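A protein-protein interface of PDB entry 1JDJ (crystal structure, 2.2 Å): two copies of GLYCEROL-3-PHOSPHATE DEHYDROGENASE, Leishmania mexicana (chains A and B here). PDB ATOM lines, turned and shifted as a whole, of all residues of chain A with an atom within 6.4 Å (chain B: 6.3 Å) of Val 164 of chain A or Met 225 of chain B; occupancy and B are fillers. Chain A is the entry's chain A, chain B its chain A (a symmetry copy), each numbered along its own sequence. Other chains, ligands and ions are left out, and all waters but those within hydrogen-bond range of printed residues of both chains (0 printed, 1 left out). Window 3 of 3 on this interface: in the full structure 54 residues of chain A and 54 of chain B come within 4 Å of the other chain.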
ATOM      1  N   LYS A  36      -6.809  -0.615  15.919  1.00  0.00           N
ATOM      2  CA  LYS A  36      -7.320  -1.056  14.624  1.00  0.00           C
ATOM      3  C   LYS A  36      -6.203  -1.372  13.648  1.00  0.00           C
ATOM      4  O   LYS A  36      -6.457  -1.803  12.522  1.00  0.00           O
ATOM      5  CB  LYS A  36      -8.217   0.020  14.011  1.00  0.00           C
ATOM      6  CG  LYS A  36      -9.347   0.471  14.911  1.00  0.00           C
ATOM      7  CD  LYS A  36     -10.042   1.698  14.341  1.00  0.00           C
ATOM      8  CE  LYS A  36     -11.112   2.206  15.291  1.00  0.00           C
ATOM      9  NZ  LYS A  36     -11.800   3.412  14.767  1.00  0.00           N
ATOM     10  N   ILE A 158     -12.522  12.836  21.776  1.00  0.00           N
ATOM     11  CA  ILE A 158     -13.751  12.057  21.709  1.00  0.00           C
ATOM     12  C   ILE A 158     -14.021  11.590  20.278  1.00  0.00           C
ATOM     13  O   ILE A 158     -14.280  10.407  20.042  1.00  0.00           O
ATOM     14  CB  ILE A 158     -14.964  12.868  22.248  1.00  0.00           C
ATOM     15  CG1 ILE A 158     -16.239  12.028  22.145  1.00  0.00           C
ATOM     16  CG2 ILE A 158     -15.119  14.172  21.477  1.00  0.00           C
ATOM     17  CD1 ILE A 158     -16.198  10.764  22.969  1.00  0.00           C
ATOM     18  N   GLU A 159     -13.942  12.508  19.318  1.00  0.00           N
ATOM     19  CA  GLU A 159     -14.177  12.147  17.925  1.00  0.00           C
ATOM     20  C   GLU A 159     -13.161  11.124  17.422  1.00  0.00           C
ATOM     21  O   GLU A 159     -13.516  10.175  16.721  1.00  0.00           O
ATOM     22  CB  GLU A 159     -14.154  13.400  17.040  1.00  0.00           C
ATOM     23  CG  GLU A 159     -15.446  14.212  17.104  1.00  0.00           C
ATOM     24  CD  GLU A 159     -15.368  15.519  16.331  1.00  0.00           C
ATOM     25  OE1 GLU A 159     -14.834  15.521  15.204  1.00  0.00           O
ATOM     26  OE2 GLU A 159     -15.857  16.545  16.845  1.00  0.00           O
ATOM     27  N   VAL A 160     -11.895  11.315  17.775  1.00  0.00           N
ATOM     28  CA  VAL A 160     -10.871  10.374  17.345  1.00  0.00           C
ATOM     29  C   VAL A 160     -11.107   9.004  17.988  1.00  0.00           C
ATOM     30  O   VAL A 160     -11.062   7.982  17.312  1.00  0.00           O
ATOM     31  CB  VAL A 160      -9.446  10.869  17.717  1.00  0.00           C
ATOM     32  CG1 VAL A 160      -8.416   9.820  17.330  1.00  0.00           C
ATOM     33  CG2 VAL A 160      -9.143  12.196  17.001  1.00  0.00           C
ATOM     34  N   ALA A 161     -11.381   8.994  19.290  1.00  0.00           N
ATOM     35  CA  ALA A 161     -11.597   7.746  20.013  1.00  0.00           C
ATOM     36  C   ALA A 161     -12.771   6.926  19.479  1.00  0.00           C
ATOM     37  O   ALA A 161     -12.706   5.699  19.448  1.00  0.00           O
ATOM     38  CB  ALA A 161     -11.790   8.033  21.499  1.00  0.00           C
ATOM     39  N   THR A 162     -13.833   7.598  19.044  1.00  0.00           N
ATOM     40  CA  THR A 162     -15.004   6.899  18.524  1.00  0.00           C
ATOM     41  C   THR A 162     -14.995   6.694  17.009  1.00  0.00           C
ATOM     42  O   THR A 162     -15.990   6.266  16.427  1.00  0.00           O
ATOM     43  CB  THR A 162     -16.305   7.612  18.938  1.00  0.00           C
ATOM     44  OG1 THR A 162     -16.245   8.984  18.550  1.00  0.00           O
ATOM     45  CG2 THR A 162     -16.494   7.538  20.447  1.00  0.00           C
ATOM     46  N   GLY A 163     -13.870   6.996  16.372  1.00  0.00           N
ATOM     47  CA  GLY A 163     -13.760   6.802  14.936  1.00  0.00           C
ATOM     48  C   GLY A 163     -14.451   7.791  14.012  1.00  0.00           C
ATOM     49  O   GLY A 163     -14.639   7.503  12.832  1.00  0.00           O
ATOM     50  N   VAL A 164     -14.842   8.948  14.529  1.00  0.00           N
ATOM     51  CA  VAL A 164     -15.487   9.956  13.696  1.00  0.00           C
ATOM     52  C   VAL A 164     -14.386  10.563  12.816  1.00  0.00           C
ATOM     53  O   VAL A 164     -13.316  10.907  13.313  1.00  0.00           O
ATOM     54  CB  VAL A 164     -16.140  11.048  14.558  1.00  0.00           C
ATOM     55  CG1 VAL A 164     -16.855  12.049  13.677  1.00  0.00           C
ATOM     56  CG2 VAL A 164     -17.118  10.409  15.543  1.00  0.00           C
ATOM     57  N   PHE A 165     -14.660  10.686  11.516  1.00  0.00           N
ATOM     58  CA  PHE A 165     -13.693  11.193  10.545  1.00  0.00           C
ATOM     59  C   PHE A 165     -12.763  12.308  11.016  1.00  0.00           C
ATOM     60  O   PHE A 165     -13.207  13.398  11.378  1.00  0.00           O
ATOM     61  CB  PHE A 165     -14.384  11.668   9.273  1.00  0.00           C
ATOM     62  CG  PHE A 165     -13.424  11.946   8.165  1.00  0.00           C
ATOM     63  CD1 PHE A 165     -12.782  10.894   7.513  1.00  0.00           C
ATOM     64  CD2 PHE A 165     -13.097  13.252   7.820  1.00  0.00           C
ATOM     65  CE1 PHE A 165     -11.823  11.142   6.535  1.00  0.00           C
ATOM     66  CE2 PHE A 165     -12.139  13.512   6.843  1.00  0.00           C
ATOM     67  CZ  PHE A 165     -11.500  12.454   6.199  1.00  0.00           C
ATOM     68  N   THR A 166     -11.465  12.028  10.953  1.00  0.00           N
ATOM     69  CA  THR A 166     -10.452  12.969  11.395  1.00  0.00           C
ATOM     70  C   THR A 166      -9.209  12.974  10.509  1.00  0.00           C
ATOM     71  O   THR A 166      -8.777  11.927  10.023  1.00  0.00           O
ATOM     72  CB  THR A 166     -10.035  12.637  12.836  1.00  0.00           C
ATOM     73  OG1 THR A 166     -11.179  12.756  13.691  1.00  0.00           O
ATOM     74  CG2 THR A 166      -8.933  13.588  13.322  1.00  0.00           C
ATOM     75  N   SER A 191     -11.053   6.413   8.429  1.00  0.00           N
ATOM     76  CA  SER A 191     -11.697   7.298   9.398  1.00  0.00           C
ATOM     77  C   SER A 191     -10.658   8.193  10.083  1.00  0.00           C
ATOM     78  O   SER A 191     -11.003   9.205  10.699  1.00  0.00           O
ATOM     79  CB  SER A 191     -12.451   6.477  10.452  1.00  0.00           C
ATOM     80  OG  SER A 191     -11.574   5.627  11.176  1.00  0.00           O
ATOM     81  N   PHE A 192      -9.390   7.802   9.989  1.00  0.00           N
ATOM     82  CA  PHE A 192      -8.286   8.574  10.565  1.00  0.00           C
ATOM     83  C   PHE A 192      -7.273   8.629   9.430  1.00  0.00           C
ATOM     84  O   PHE A 192      -6.618   7.633   9.130  1.00  0.00           O
ATOM     85  CB  PHE A 192      -7.685   7.862  11.783  1.00  0.00           C
ATOM     86  CG  PHE A 192      -6.812   8.749  12.649  1.00  0.00           C
ATOM     87  CD1 PHE A 192      -7.381   9.685  13.513  1.00  0.00           C
ATOM     88  CD2 PHE A 192      -5.423   8.647  12.599  1.00  0.00           C
ATOM     89  CE1 PHE A 192      -6.577  10.511  14.320  1.00  0.00           C
ATOM     90  CE2 PHE A 192      -4.611   9.463  13.400  1.00  0.00           C
ATOM     91  CZ  PHE A 192      -5.191  10.396  14.261  1.00  0.00           C
ATOM     92  N   VAL B 219     -22.969  18.805   4.452  1.00  0.00           N
ATOM     93  CA  VAL B 219     -22.977  17.387   4.120  1.00  0.00           C
ATOM     94  C   VAL B 219     -22.265  16.581   5.201  1.00  0.00           C
ATOM     95  O   VAL B 219     -22.792  15.583   5.691  1.00  0.00           O
ATOM     96  CB  VAL B 219     -22.284  17.126   2.768  1.00  0.00           C
ATOM     97  CG1 VAL B 219     -22.184  15.633   2.514  1.00  0.00           C
ATOM     98  CG2 VAL B 219     -23.061  17.793   1.647  1.00  0.00           C
ATOM     99  N   ALA B 220     -21.066  17.025   5.567  1.00  0.00           N
ATOM    100  CA  ALA B 220     -20.279  16.352   6.590  1.00  0.00           C
ATOM    101  C   ALA B 220     -21.084  16.194   7.878  1.00  0.00           C
ATOM    102  O   ALA B 220     -21.064  15.133   8.501  1.00  0.00           O
ATOM    103  CB  ALA B 220     -18.994  17.137   6.861  1.00  0.00           C
ATOM    104  N   ASN B 221     -21.790  17.249   8.274  1.00  0.00           N
ATOM    105  CA  ASN B 221     -22.605  17.201   9.482  1.00  0.00           C
ATOM    106  C   ASN B 221     -23.777  16.227   9.326  1.00  0.00           C
ATOM    107  O   ASN B 221     -24.005  15.370  10.184  1.00  0.00           O
ATOM    108  CB  ASN B 221     -23.120  18.603   9.823  1.00  0.00           C
ATOM    109  CG  ASN B 221     -24.101  18.600  10.983  1.00  0.00           C
ATOM    110  OD1 ASN B 221     -25.263  18.226  10.827  1.00  0.00           O
ATOM    111  ND2 ASN B 221     -23.632  19.009  12.159  1.00  0.00           N
ATOM    112  N   GLY B 222     -24.516  16.351   8.231  1.00  0.00           N
ATOM    113  CA  GLY B 222     -25.638  15.456   8.011  1.00  0.00           C
ATOM    114  C   GLY B 222     -25.188  14.016   7.826  1.00  0.00           C
ATOM    115  O   GLY B 222     -25.987  13.087   7.917  1.00  0.00           O
ATOM    116  N   LEU B 223     -23.897  13.828   7.576  1.00  0.00           N
ATOM    117  CA  LEU B 223     -23.347  12.497   7.360  1.00  0.00           C
ATOM    118  C   LEU B 223     -22.907  11.843   8.672  1.00  0.00           C
ATOM    119  O   LEU B 223     -22.499  10.683   8.694  1.00  0.00           O
ATOM    120  CB  LEU B 223     -22.168  12.591   6.388  1.00  0.00           C
ATOM    121  CG  LEU B 223     -22.109  11.620   5.207  1.00  0.00           C
ATOM    122  CD1 LEU B 223     -23.432  11.602   4.471  1.00  0.00           C
ATOM    123  CD2 LEU B 223     -20.988  12.040   4.271  1.00  0.00           C
ATOM    124  N   GLY B 224     -22.995  12.591   9.766  1.00  0.00           N
ATOM    125  CA  GLY B 224     -22.608  12.056  11.057  1.00  0.00           C
ATOM    126  C   GLY B 224     -21.228  12.476  11.534  1.00  0.00           C
ATOM    127  O   GLY B 224     -20.829  12.135  12.647  1.00  0.00           O
ATOM    128  N   MET B 225     -20.498  13.218  10.707  1.00  0.00           N
ATOM    129  CA  MET B 225     -19.158  13.668  11.074  1.00  0.00           C
ATOM    130  C   MET B 225     -19.205  14.812  12.083  1.00  0.00           C
ATOM    131  O   MET B 225     -20.249  15.434  12.283  1.00  0.00           O
ATOM    132  CB  MET B 225     -18.390  14.091   9.825  1.00  0.00           C
ATOM    133  CG  MET B 225     -18.416  13.041   8.729  1.00  0.00           C
ATOM    134  SD  MET B 225     -17.419  13.475   7.297  1.00  0.00           S
ATOM    135  CE  MET B 225     -16.828  11.888   6.814  1.00  0.00           C
ATOM    136  N   GLY B 226     -18.070  15.087  12.716  1.00  0.00           N
ATOM    137  CA  GLY B 226     -18.019  16.138  13.712  1.00  0.00           C
ATOM    138  C   GLY B 226     -17.191  17.345  13.322  1.00  0.00           C
ATOM    139  O   GLY B 226     -17.070  17.672  12.146  1.00  0.00           O
ATOM    140  N   LEU B 227     -16.604  17.996  14.320  1.00  0.00           N
ATOM    141  CA  LEU B 227     -15.803  19.191  14.099  1.00  0.00           C
ATOM    142  C   LEU B 227     -14.402  18.959  13.539  1.00  0.00           C
ATOM    143  O   LEU B 227     -13.803  19.880  12.971  1.00  0.00           O
ATOM    144  CB  LEU B 227     -15.730  19.994  15.395  1.00  0.00           C
ATOM    145  CG  LEU B 227     -17.119  20.387  15.906  1.00  0.00           C
ATOM    146  CD1 LEU B 227     -17.008  21.027  17.281  1.00  0.00           C
ATOM    147  CD2 LEU B 227     -17.772  21.335  14.913  1.00  0.00           C
ATOM    148  N   ASN B 228     -13.867  17.752  13.703  1.00  0.00           N
ATOM    149  CA  ASN B 228     -12.545  17.466  13.161  1.00  0.00           C
ATOM    150  C   ASN B 228     -12.698  17.476  11.641  1.00  0.00           C
ATOM    151  O   ASN B 228     -11.874  18.041  10.920  1.00  0.00           O
ATOM    152  CB  ASN B 228     -12.025  16.087  13.613  1.00  0.00           C
ATOM    153  CG  ASN B 228     -11.671  16.037  15.095  1.00  0.00           C
ATOM    154  OD1 ASN B 228     -11.596  17.062  15.772  1.00  0.00           O
ATOM    155  ND2 ASN B 228     -11.436  14.832  15.600  1.00  0.00           N
ATOM    156  N   ALA B 229     -13.775  16.862  11.168  1.00  0.00           N
ATOM    157  CA  ALA B 229     -14.046  16.783   9.741  1.00  0.00           C
ATOM    158  C   ALA B 229     -14.233  18.168   9.135  1.00  0.00           C
ATOM    159  O   ALA B 229     -13.738  18.445   8.042  1.00  0.00           O
ATOM    160  CB  ALA B 229     -15.293  15.932   9.491  1.00  0.00           C
ATOM    161  N   ARG B 230     -14.957  19.028   9.846  1.00  0.00           N
ATOM    162  CA  ARG B 230     -15.206  20.385   9.376  1.00  0.00           C
ATOM    163  C   ARG B 230     -13.892  21.155   9.248  1.00  0.00           C
ATOM    164  O   ARG B 230     -13.683  21.883   8.277  1.00  0.00           O
ATOM    165  CB  ARG B 230     -16.148  21.122  10.337  1.00  0.00           C
ATOM    166  CG  ARG B 230     -16.494  22.537   9.885  1.00  0.00           C
ATOM    167  CD  ARG B 230     -17.303  23.280  10.940  1.00  0.00           C
ATOM    168  NE  ARG B 230     -18.588  22.635  11.187  1.00  0.00           N
ATOM    169  CZ  ARG B 230     -19.455  23.032  12.110  1.00  0.00           C
ATOM    170  NH1 ARG B 230     -19.175  24.077  12.876  1.00  0.00           N
ATOM    171  NH2 ARG B 230     -20.600  22.381  12.268  1.00  0.00           N
ATOM    172  N   LEU B 339     -17.684  10.794  -0.698  1.00  0.00           N
ATOM    173  CA  LEU B 339     -16.661  10.797   0.334  1.00  0.00           C
ATOM    174  C   LEU B 339     -15.587   9.747   0.031  1.00  0.00           C
ATOM    175  O   LEU B 339     -14.390  10.043   0.062  1.00  0.00           O
ATOM    176  CB  LEU B 339     -17.305  10.501   1.691  1.00  0.00           C
ATOM    177  CG  LEU B 339     -16.614  10.978   2.974  1.00  0.00           C
ATOM    178  CD1 LEU B 339     -17.105  10.119   4.127  1.00  0.00           C
ATOM    179  CD2 LEU B 339     -15.107  10.873   2.856  1.00  0.00           C
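Among the printed residues, pairs that only touch across the chains: Val 164 of chain A with Gly 226 of chain B, Phe 165 of chain A with Met 225 of chain B, Phe 165 of chain A with Ala 229 of chain B, Glu 159 of chain A with Gly 226 of chain B, Phe 165 of chain A with Asn 228 of chain B, Val 160 of chain A with Asn 228 of chain B and Val 164 of chain A with Met 225 of chain B.
Of the 12 printed residues of chain A, 5 touch a printed residue of chain B. Printed residues of chain A that touch a printed residue of chain B: Glu 159, Val 160, Val 164, Phe 165 and Thr 166. Of the 13 printed residues of chain B, 5 touch a printed residue of chain A.
The backbone NH (N) of Leu 227 of chain B lies within hydrogen-bond range of the side-chain carboxylate (OE2) of Glu 159 of chain A (3.0 Å). The backbone NH of Asn 228 of chain B lies within hydrogen-bond range of the side-chain carboxylate of Glu 159 of chain A, 2.9 Å away. The side-chain amide nitrogen (ND2) of Asn 228 of chain B lies within hydrogen-bond range of the side-chain hydroxyl (OG1) of Thr 166 of chain A (2.8 Å).
Of the printed residues of chain B, Glu 159 of chain A touches Gly 226 (3.5 Å), Leu 227 (3.0 Å) and Asn 228 (2.9 Å). Of the printed residues of chain B, Val 164 of chain A touches Met 225 and Gly 226. Of the printed residues of chain B, Phe 165 of chain A touches Met 225, Asn 228 and Ala 229. Met 225 of chain B touches just these residues of chain A: Val 164 and Phe 165. Printed residues of chain A within 4 Å of Gly 226 of chain B: Glu 159 (3.5 Å) and Val 164 (3.4 Å). Of the printed residues of chain A, Asn 228 of chain B touches Glu 159 (2.9 Å), Val 160 (3.8 Å), Phe 165 (3.7 Å) and Thr 166 (2.8 Å). The nearest residue of chain B that does not touch Val 164 of chain A is Gly 224 of chain B (4.1 Å). The nearest residue of chain A that does not touch Met 225 of chain B is Glu 159 of chain A (5.4 Å). The nearest printed residue of chain A that does not touch Leu 227 of chain B is Val 164 of chain A (6.0 Å).
No position is printed for both chains. Of the 10 pairs that touch across the chains among the printed residues, none has its exchanged pair printed and touching as well.
The backbone carbonyl oxygen (O) of Glu 159 of chain A is in hydrogen-bond range of the side-chain hydroxyl (OG1) of Thr 162 of chain A (3.5 Å). N of Val 164 of chain A sits at hydrogen-bond distance from O of Glu 159 of chain A (2.8 Å). The backbone carbonyl oxygen (O) of Val 164 of chain A is in hydrogen-bond range of the side-chain hydroxyl (OG1) of Thr 166 of chain A, 2.9 Å away. O of Ser 191 of chain A sits at hydrogen-bond distance from N of Thr 166 of chain A, 2.9 Å away. The backbone NH of Met 225 of chain B is in hydrogen-bond range of the backbone carbonyl oxygen of Ala 220 of chain B (3.0 Å).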
